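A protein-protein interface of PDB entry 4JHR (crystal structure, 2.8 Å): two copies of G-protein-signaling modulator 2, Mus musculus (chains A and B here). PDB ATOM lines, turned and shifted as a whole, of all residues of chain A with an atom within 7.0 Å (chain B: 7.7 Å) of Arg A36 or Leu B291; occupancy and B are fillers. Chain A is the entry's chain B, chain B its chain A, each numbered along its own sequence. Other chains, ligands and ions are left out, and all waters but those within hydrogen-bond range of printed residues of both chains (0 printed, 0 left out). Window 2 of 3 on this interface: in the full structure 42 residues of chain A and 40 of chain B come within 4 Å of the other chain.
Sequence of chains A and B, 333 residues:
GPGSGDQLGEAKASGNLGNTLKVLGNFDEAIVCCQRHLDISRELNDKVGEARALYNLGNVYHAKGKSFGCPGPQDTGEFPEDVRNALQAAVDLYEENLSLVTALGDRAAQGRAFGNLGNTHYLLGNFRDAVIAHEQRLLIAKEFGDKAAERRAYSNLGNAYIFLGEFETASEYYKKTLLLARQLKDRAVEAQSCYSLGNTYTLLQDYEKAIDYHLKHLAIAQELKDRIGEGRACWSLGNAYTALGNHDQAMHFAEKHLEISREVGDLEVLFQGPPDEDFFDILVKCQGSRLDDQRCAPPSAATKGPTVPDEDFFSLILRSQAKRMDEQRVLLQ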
ATOM      1  N   ALA A  30      30.325 -12.806  19.377  1.00  0.00           N
ATOM      2  CA  ALA A  30      29.010 -12.167  19.362  1.00  0.00           C
ATOM      3  C   ALA A  30      28.993 -10.765  19.981  1.00  0.00           C
ATOM      4  O   ALA A  30      28.418  -9.837  19.403  1.00  0.00           O
ATOM      5  CB  ALA A  30      27.986 -13.054  20.013  1.00  0.00           C
ATOM      6  N   ILE A  31      29.620 -10.604  21.146  1.00  0.00           N
ATOM      7  CA  ILE A  31      29.530  -9.329  21.850  1.00  0.00           C
ATOM      8  C   ILE A  31      30.209  -8.223  21.052  1.00  0.00           C
ATOM      9  O   ILE A  31      29.714  -7.098  20.991  1.00  0.00           O
ATOM     10  CB  ILE A  31      30.099  -9.393  23.300  1.00  0.00           C
ATOM     11  CG1 ILE A  31      30.070  -8.017  23.939  1.00  0.00           C
ATOM     12  CG2 ILE A  31      31.535  -9.884  23.328  1.00  0.00           C
ATOM     13  CD1 ILE A  31      31.158  -7.814  24.963  1.00  0.00           C
ATOM     14  N   VAL A  32      31.334  -8.531  20.418  1.00  0.00           N
ATOM     15  CA  VAL A  32      32.023  -7.468  19.693  1.00  0.00           C
ATOM     16  C   VAL A  32      31.224  -7.020  18.483  1.00  0.00           C
ATOM     17  O   VAL A  32      31.139  -5.817  18.206  1.00  0.00           O
ATOM     18  CB  VAL A  32      33.528  -7.741  19.398  1.00  0.00           C
ATOM     19  CG1 VAL A  32      34.068  -8.954  20.111  1.00  0.00           C
ATOM     20  CG2 VAL A  32      33.896  -7.607  17.934  1.00  0.00           C
ATOM     21  N   CYS A  33      30.592  -7.981  17.811  1.00  0.00           N
ATOM     22  CA  CYS A  33      29.656  -7.668  16.732  1.00  0.00           C
ATOM     23  C   CYS A  33      28.546  -6.704  17.153  1.00  0.00           C
ATOM     24  O   CYS A  33      28.274  -5.720  16.461  1.00  0.00           O
ATOM     25  CB  CYS A  33      29.040  -8.950  16.177  1.00  0.00           C
ATOM     26  SG  CYS A  33      30.258 -10.103  15.526  1.00  0.00           S
ATOM     27  N   CYS A  34      27.893  -6.973  18.276  1.00  0.00           N
ATOM     28  CA  CYS A  34      26.811  -6.084  18.681  1.00  0.00           C
ATOM     29  C   CYS A  34      27.416  -4.755  19.021  1.00  0.00           C
ATOM     30  O   CYS A  34      26.840  -3.715  18.720  1.00  0.00           O
ATOM     31  CB  CYS A  34      26.039  -6.609  19.886  1.00  0.00           C
ATOM     32  SG  CYS A  34      25.479  -8.315  19.750  1.00  0.00           S
ATOM     33  N   GLN A  35      28.592  -4.796  19.638  1.00  0.00           N
ATOM     34  CA  GLN A  35      29.285  -3.577  20.010  1.00  0.00           C
ATOM     35  C   GLN A  35      29.577  -2.736  18.764  1.00  0.00           C
ATOM     36  O   GLN A  35      29.308  -1.516  18.744  1.00  0.00           O
ATOM     37  CB  GLN A  35      30.568  -3.897  20.765  1.00  0.00           C
ATOM     38  CG  GLN A  35      31.177  -2.687  21.420  1.00  0.00           C
ATOM     39  CD  GLN A  35      30.224  -2.037  22.404  1.00  0.00           C
ATOM     40  OE1 GLN A  35      29.797  -2.667  23.369  1.00  0.00           O
ATOM     41  NE2 GLN A  35      29.880  -0.775  22.163  1.00  0.00           N
ATOM     42  N   ARG A  36      30.090  -3.401  17.723  1.00  0.00           N
ATOM     43  CA  ARG A  36      30.278  -2.760  16.422  1.00  0.00           C
ATOM     44  C   ARG A  36      28.976  -2.128  15.965  1.00  0.00           C
ATOM     45  O   ARG A  36      28.927  -0.934  15.664  1.00  0.00           O
ATOM     46  CB  ARG A  36      30.761  -3.770  15.381  1.00  0.00           C
ATOM     47  N   HIS A  37      27.920  -2.933  15.945  1.00  0.00           N
ATOM     48  CA  HIS A  37      26.599  -2.498  15.489  1.00  0.00           C
ATOM     49  C   HIS A  37      26.138  -1.259  16.240  1.00  0.00           C
ATOM     50  O   HIS A  37      25.711  -0.268  15.633  1.00  0.00           O
ATOM     51  CB  HIS A  37      25.594  -3.635  15.690  1.00  0.00           C
ATOM     52  CG  HIS A  37      24.187  -3.301  15.292  1.00  0.00           C
ATOM     53  ND1 HIS A  37      23.854  -2.172  14.568  1.00  0.00           N
ATOM     54  CD2 HIS A  37      23.023  -3.964  15.506  1.00  0.00           C
ATOM     55  CE1 HIS A  37      22.549  -2.149  14.363  1.00  0.00           C
ATOM     56  NE2 HIS A  37      22.021  -3.229  14.919  1.00  0.00           N
ATOM     57  N   LEU A  38      26.233  -1.329  17.564  1.00  0.00           N
ATOM     58  CA  LEU A  38      25.815  -0.236  18.428  1.00  0.00           C
ATOM     59  C   LEU A  38      26.652   1.021  18.175  1.00  0.00           C
ATOM     60  O   LEU A  38      26.106   2.124  17.993  1.00  0.00           O
ATOM     61  CB  LEU A  38      25.929  -0.691  19.878  1.00  0.00           C
ATOM     62  CG  LEU A  38      25.771   0.286  21.035  1.00  0.00           C
ATOM     63  CD1 LEU A  38      24.464   0.978  20.943  1.00  0.00           C
ATOM     64  CD2 LEU A  38      25.867  -0.510  22.323  1.00  0.00           C
ATOM     65  N   ASP A  39      27.973   0.826  18.165  1.00  0.00           N
ATOM     66  CA  ASP A  39      28.938   1.869  17.842  1.00  0.00           C
ATOM     67  C   ASP A  39      28.485   2.673  16.638  1.00  0.00           C
ATOM     68  O   ASP A  39      28.350   3.898  16.709  1.00  0.00           O
ATOM     69  CB  ASP A  39      30.263   1.212  17.465  1.00  0.00           C
ATOM     70  CG  ASP A  39      31.211   1.053  18.638  1.00  0.00           C
ATOM     71  OD1 ASP A  39      30.786   1.205  19.811  1.00  0.00           O
ATOM     72  OD2 ASP A  39      32.396   0.766  18.360  1.00  0.00           O
ATOM     73  N   ILE A  40      28.271   1.957  15.534  1.00  0.00           N
ATOM     74  CA  ILE A  40      27.854   2.526  14.260  1.00  0.00           C
ATOM     75  C   ILE A  40      26.517   3.251  14.394  1.00  0.00           C
ATOM     76  O   ILE A  40      26.342   4.348  13.880  1.00  0.00           O
ATOM     77  CB  ILE A  40      27.744   1.400  13.185  1.00  0.00           C
ATOM     78  CG1 ILE A  40      29.092   1.172  12.490  1.00  0.00           C
ATOM     79  CG2 ILE A  40      26.628   1.683  12.152  1.00  0.00           C
ATOM     80  CD1 ILE A  40      30.175   0.721  13.402  1.00  0.00           C
ATOM     81  N   SER A  41      25.572   2.645  15.098  1.00  0.00           N
ATOM     82  CA  SER A  41      24.216   3.171  15.132  1.00  0.00           C
ATOM     83  C   SER A  41      24.204   4.483  15.876  1.00  0.00           C
ATOM     84  O   SER A  41      23.368   5.347  15.628  1.00  0.00           O
ATOM     85  CB  SER A  41      23.282   2.179  15.817  1.00  0.00           C
ATOM     86  OG  SER A  41      23.604   0.847  15.443  1.00  0.00           O
ATOM     87  N   ARG A  42      25.147   4.618  16.801  1.00  0.00           N
ATOM     88  CA  ARG A  42      25.297   5.838  17.585  1.00  0.00           C
ATOM     89  C   ARG A  42      25.915   6.929  16.724  1.00  0.00           C
ATOM     90  O   ARG A  42      25.466   8.079  16.736  1.00  0.00           O
ATOM     91  CB  ARG A  42      26.163   5.564  18.810  1.00  0.00           C
ATOM     92  CG  ARG A  42      25.416   4.858  19.924  1.00  0.00           C
ATOM     93  CD  ARG A  42      26.313   4.480  21.107  1.00  0.00           C
ATOM     94  NE  ARG A  42      25.509   4.122  22.281  1.00  0.00           N
ATOM     95  CZ  ARG A  42      25.956   3.433  23.329  1.00  0.00           C
ATOM     96  NH1 ARG A  42      27.212   3.001  23.372  1.00  0.00           N
ATOM     97  NH2 ARG A  42      25.138   3.161  24.333  1.00  0.00           N
ATOM     98  N   ALA A  53      20.621  -3.024  18.842  1.00  0.00           N
ATOM     99  CA  ALA A  53      21.936  -3.494  19.288  1.00  0.00           C
ATOM    100  C   ALA A  53      21.973  -3.680  20.789  1.00  0.00           C
ATOM    101  O   ALA A  53      22.642  -4.573  21.288  1.00  0.00           O
ATOM    102  CB  ALA A  53      23.017  -2.553  18.864  1.00  0.00           C
ATOM    103  N   ASN A  56      20.186  -6.941  21.469  1.00  0.00           N
ATOM    104  CA  ASN A  56      21.019  -8.067  21.071  1.00  0.00           C
ATOM    105  C   ASN A  56      22.109  -8.292  22.091  1.00  0.00           C
ATOM    106  O   ASN A  56      22.319  -9.420  22.540  1.00  0.00           O
ATOM    107  CB  ASN A  56      21.606  -7.874  19.677  1.00  0.00           C
ATOM    108  CG  ASN A  56      20.550  -7.907  18.602  1.00  0.00           C
ATOM    109  OD1 ASN A  56      19.545  -8.619  18.723  1.00  0.00           O
ATOM    110  ND2 ASN A  56      20.747  -7.112  17.550  1.00  0.00           N
ATOM    111  N   ASP B 281      22.542 -15.644  14.143  1.00  0.00           N
ATOM    112  CA  ASP B 281      21.956 -14.503  13.433  1.00  0.00           C
ATOM    113  C   ASP B 281      22.655 -13.194  13.766  1.00  0.00           C
ATOM    114  O   ASP B 281      22.203 -12.132  13.386  1.00  0.00           O
ATOM    115  CB  ASP B 281      20.442 -14.424  13.696  1.00  0.00           C
ATOM    116  CG  ASP B 281      19.644 -15.499  12.917  1.00  0.00           C
ATOM    117  OD1 ASP B 281      20.161 -15.985  11.879  1.00  0.00           O
ATOM    118  OD2 ASP B 281      18.503 -15.857  13.323  1.00  0.00           O
ATOM    119  N   ILE B 282      23.760 -13.287  14.499  1.00  0.00           N
ATOM    120  CA  ILE B 282      24.623 -12.142  14.774  1.00  0.00           C
ATOM    121  C   ILE B 282      25.970 -12.338  14.097  1.00  0.00           C
ATOM    122  O   ILE B 282      26.478 -11.421  13.438  1.00  0.00           O
ATOM    123  CB  ILE B 282      24.867 -11.965  16.278  1.00  0.00           C
ATOM    124  CG1 ILE B 282      23.692 -11.237  16.927  1.00  0.00           C
ATOM    125  CG2 ILE B 282      26.145 -11.175  16.538  1.00  0.00           C
ATOM    126  CD1 ILE B 282      23.841 -11.099  18.411  1.00  0.00           C
ATOM    127  N   VAL B 284      26.749 -14.182  11.631  1.00  0.00           N
ATOM    128  CA  VAL B 284      26.613 -14.335  10.193  1.00  0.00           C
ATOM    129  C   VAL B 284      26.465 -12.970   9.482  1.00  0.00           C
ATOM    130  O   VAL B 284      26.668 -12.846   8.270  1.00  0.00           O
ATOM    131  CB  VAL B 284      25.442 -15.322   9.930  1.00  0.00           C
ATOM    132  CG1 VAL B 284      24.350 -14.750   9.047  1.00  0.00           C
ATOM    133  CG2 VAL B 284      25.975 -16.638   9.422  1.00  0.00           C
ATOM    134  N   LYS B 285      26.139 -11.949  10.267  1.00  0.00           N
ATOM    135  CA  LYS B 285      25.956 -10.599   9.776  1.00  0.00           C
ATOM    136  C   LYS B 285      26.959  -9.685  10.472  1.00  0.00           C
ATOM    137  O   LYS B 285      26.582  -8.676  11.075  1.00  0.00           O
ATOM    138  CB  LYS B 285      24.534 -10.129  10.077  1.00  0.00           C
ATOM    139  CG  LYS B 285      23.659  -9.917   8.859  1.00  0.00           C
ATOM    140  CD  LYS B 285      23.081 -11.246   8.358  1.00  0.00           C
ATOM    141  CE  LYS B 285      22.062 -11.047   7.229  1.00  0.00           C
ATOM    142  NZ  LYS B 285      22.608 -10.250   6.067  1.00  0.00           N
ATOM    143  N   CYS B 286      28.236 -10.049  10.399  1.00  0.00           N
ATOM    144  CA  CYS B 286      29.280  -9.277  11.069  1.00  0.00           C
ATOM    145  C   CYS B 286      30.352  -8.845  10.079  1.00  0.00           C
ATOM    146  O   CYS B 286      31.522  -8.715  10.440  1.00  0.00           O
ATOM    147  CB  CYS B 286      29.924 -10.126  12.146  1.00  0.00           C
ATOM    148  SG  CYS B 286      30.306  -9.251  13.668  1.00  0.00           S
ATOM    149  N   GLN B 287      29.942  -8.634   8.831  1.00  0.00           N
ATOM    150  CA  GLN B 287      30.862  -8.295   7.751  1.00  0.00           C
ATOM    151  C   GLN B 287      30.771  -6.819   7.353  1.00  0.00           C
ATOM    152  O   GLN B 287      29.730  -6.330   6.894  1.00  0.00           O
ATOM    153  CB  GLN B 287      30.618  -9.194   6.535  1.00  0.00           C
ATOM    154  N   GLY B 288      31.881  -6.114   7.539  1.00  0.00           N
ATOM    155  CA  GLY B 288      31.957  -4.711   7.208  1.00  0.00           C
ATOM    156  C   GLY B 288      31.095  -3.904   8.144  1.00  0.00           C
ATOM    157  O   GLY B 288      31.008  -4.232   9.321  1.00  0.00           O
ATOM    158  N   SER B 289      30.458  -2.857   7.619  1.00  0.00           N
ATOM    159  CA  SER B 289      29.585  -1.999   8.419  1.00  0.00           C
ATOM    160  C   SER B 289      28.121  -2.059   7.972  1.00  0.00           C
ATOM    161  O   SER B 289      27.332  -1.180   8.302  1.00  0.00           O
ATOM    162  CB  SER B 289      30.106  -0.552   8.477  1.00  0.00           C
ATOM    163  OG  SER B 289      30.669  -0.121   7.247  1.00  0.00           O
ATOM    164  N   ARG B 290      27.763  -3.114   7.239  1.00  0.00           N
ATOM    165  CA  ARG B 290      26.366  -3.382   6.903  1.00  0.00           C
ATOM    166  C   ARG B 290      25.755  -4.337   7.951  1.00  0.00           C
ATOM    167  O   ARG B 290      25.498  -5.520   7.680  1.00  0.00           O
ATOM    168  CB  ARG B 290      26.308  -3.967   5.503  1.00  0.00           C
ATOM    169  CG  ARG B 290      27.448  -3.443   4.628  1.00  0.00           C
ATOM    170  CD  ARG B 290      26.936  -2.859   3.321  1.00  0.00           C
ATOM    171  NE  ARG B 290      26.740  -3.894   2.308  1.00  0.00           N
ATOM    172  CZ  ARG B 290      25.675  -3.982   1.513  1.00  0.00           C
ATOM    173  NH1 ARG B 290      24.699  -3.083   1.600  1.00  0.00           N
ATOM    174  NH2 ARG B 290      25.591  -4.968   0.625  1.00  0.00           N
ATOM    175  N   LEU B 291      25.523  -3.800   9.150  1.00  0.00           N
ATOM    176  CA  LEU B 291      25.260  -4.609  10.340  1.00  0.00           C
ATOM    177  C   LEU B 291      23.848  -4.479  10.881  1.00  0.00           C
ATOM    178  O   LEU B 291      23.536  -5.028  11.924  1.00  0.00           O
ATOM    179  CB  LEU B 291      26.226  -4.220  11.462  1.00  0.00           C
ATOM    180  CG  LEU B 291      27.721  -4.264  11.189  1.00  0.00           C
ATOM    181  CD1 LEU B 291      28.486  -3.982  12.472  1.00  0.00           C
ATOM    182  CD2 LEU B 291      28.117  -5.587  10.575  1.00  0.00           C
ATOM    183  N   ASP B 292      23.001  -3.752  10.169  1.00  0.00           N
ATOM    184  CA  ASP B 292      21.681  -3.412  10.659  1.00  0.00           C
ATOM    185  C   ASP B 292      20.787  -4.650  10.852  1.00  0.00           C
ATOM    186  O   ASP B 292      19.752  -4.581  11.532  1.00  0.00           O
ATOM    187  CB  ASP B 292      21.028  -2.408   9.708  1.00  0.00           C
ATOM    188  CG  ASP B 292      20.093  -1.442  10.429  1.00  0.00           C
ATOM    189  OD1 ASP B 292      18.932  -1.271   9.982  1.00  0.00           O
ATOM    190  OD2 ASP B 292      20.517  -0.849  11.445  1.00  0.00           O
ATOM    191  N   ASP B 293      21.189  -5.784  10.282  1.00  0.00           N
ATOM    192  CA  ASP B 293      20.328  -6.960  10.294  1.00  0.00           C
ATOM    193  C   ASP B 293      20.763  -8.057  11.272  1.00  0.00           C
ATOM    194  O   ASP B 293      20.304  -9.215  11.176  1.00  0.00           O
ATOM    195  CB  ASP B 293      20.140  -7.522   8.876  1.00  0.00           C
ATOM    196  CG  ASP B 293      21.083  -6.888   7.862  1.00  0.00           C
ATOM    197  OD1 ASP B 293      20.721  -6.850   6.658  1.00  0.00           O
ATOM    198  OD2 ASP B 293      22.182  -6.430   8.272  1.00  0.00           O
ATOM    199  N   GLN B 294      21.631  -7.697  12.215  1.00  0.00           N
ATOM    200  CA  GLN B 294      21.963  -8.602  13.312  1.00  0.00           C
ATOM    201  C   GLN B 294      20.729  -8.875  14.152  1.00  0.00           C
ATOM    202  O   GLN B 294      20.024  -7.953  14.533  1.00  0.00           O
ATOM    203  CB  GLN B 294      22.997  -7.980  14.226  1.00  0.00           C
ATOM    204  CG  GLN B 294      24.374  -7.809  13.644  1.00  0.00           C
ATOM    205  CD  GLN B 294      25.385  -7.469  14.726  1.00  0.00           C
ATOM    206  OE1 GLN B 294      25.021  -7.214  15.879  1.00  0.00           O
ATOM    207  NE2 GLN B 294      26.656  -7.484  14.369  1.00  0.00           N
ATOM    208  N   ARG B 295      20.475 -10.139  14.454  1.00  0.00           N
ATOM    209  CA  ARG B 295      19.337 -10.516  15.280  1.00  0.00           C
ATOM    210  C   ARG B 295      19.803 -11.489  16.343  1.00  0.00           C
ATOM    211  O   ARG B 295      20.732 -12.278  16.112  1.00  0.00           O
ATOM    212  CB  ARG B 295      18.245 -11.208  14.448  1.00  0.00           C
ATOM    213  CG  ARG B 295      17.334 -10.302  13.643  1.00  0.00           C
ATOM    214  CD  ARG B 295      16.798  -9.160  14.471  1.00  0.00           C
ATOM    215  NE  ARG B 295      17.480  -7.921  14.141  1.00  0.00           N
ATOM    216  CZ  ARG B 295      16.981  -6.980  13.358  1.00  0.00           C
ATOM    217  NH1 ARG B 295      15.776  -7.127  12.820  1.00  0.00           N
ATOM    218  NH2 ARG B 295      17.693  -5.888  13.124  1.00  0.00           N
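Of the 14 printed residues of chain B, 6 touch a printed residue of chain A. Hydrophobic or aromatic side chains of chain B that line the printed part of chain A: Ile B282 and Leu B291. Printed residues of chain A that touch a printed residue of chain B: Ala A30, Cys A33, Cys A34, Arg A36, His A37 and Asn A56.
SG of Cys A33 forms a disulfide with SG of Cys B286 (2.0 Å). The backbone carbonyl oxygen (O) of Cys A33 sits at hydrogen-bond distance from the side-chain amide nitrogen (NE2) of Gln B294 (3.2 Å). The backbone carbonyl oxygen (O) of Gln B294 sits at hydrogen-bond distance from the side-chain amide nitrogen (ND2) of Asn A56.
The backbone NH (N) of Arg B295 sits at hydrogen-bond distance from the backbone carbonyl oxygen (O) of Asp B281, 2.8 Å away. The backbone carbonyl oxygen of Asp B292 is in hydrogen-bond range of the guanidinium group of Arg B295, at 2.9 Å. The backbone carbonyl oxygen of Ala A30 is in hydrogen-bond range of the side-chain sulfur of Cys A34 (3.3 Å). A ring nitrogen (ND1) of His A37 lies within hydrogen-bond range of the side-chain hydroxyl (OG) of Ser A41 (3.2 Å).
Arg A36 touches just one residue of chain B: Leu B291. Of chain A, only Arg A36 (3.7 Å) and His A37 (3.7 Å) come within 4 Å of Leu B291. Of the printed residues of chain A, Arg B295 touches Asn A56 (3.7 Å). Of the printed residues of chain A, Ile B282 touches Ala A30 (3.9 Å), Cys A33 (3.7 Å) and Cys A34 (3.5 Å). Of the printed residues of chain A, Asp B292 touches His A37. The nearest residue of chain B that does not touch Arg A36 is Gln B294 (5.6 Å). The nearest residue of chain A that does not touch Leu B291 is Cys A33 (4.4 Å).
Among the printed residues, pairs that only touch across the chains: Cys A34 with Ile B282 (3.5 Å), Cys A34 with Gln B294 (3.5 Å), His A37 with Gln B294 (3.6 Å), Cys A33 with Ile B282 (3.7 Å), His A37 with Leu B291 (3.7 Å), Arg A36 with Leu B291 (3.7 Å), Asn A56 with Arg B295 (3.7 Å), His A37 with Asp B292 (3.8 Å) and Ala A30 with Ile B282 (3.9 Å).
No position is printed for both chains. Of the 12 pairs that touch across the chains among the printed residues, none has its exchanged pair printed and touching as well.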
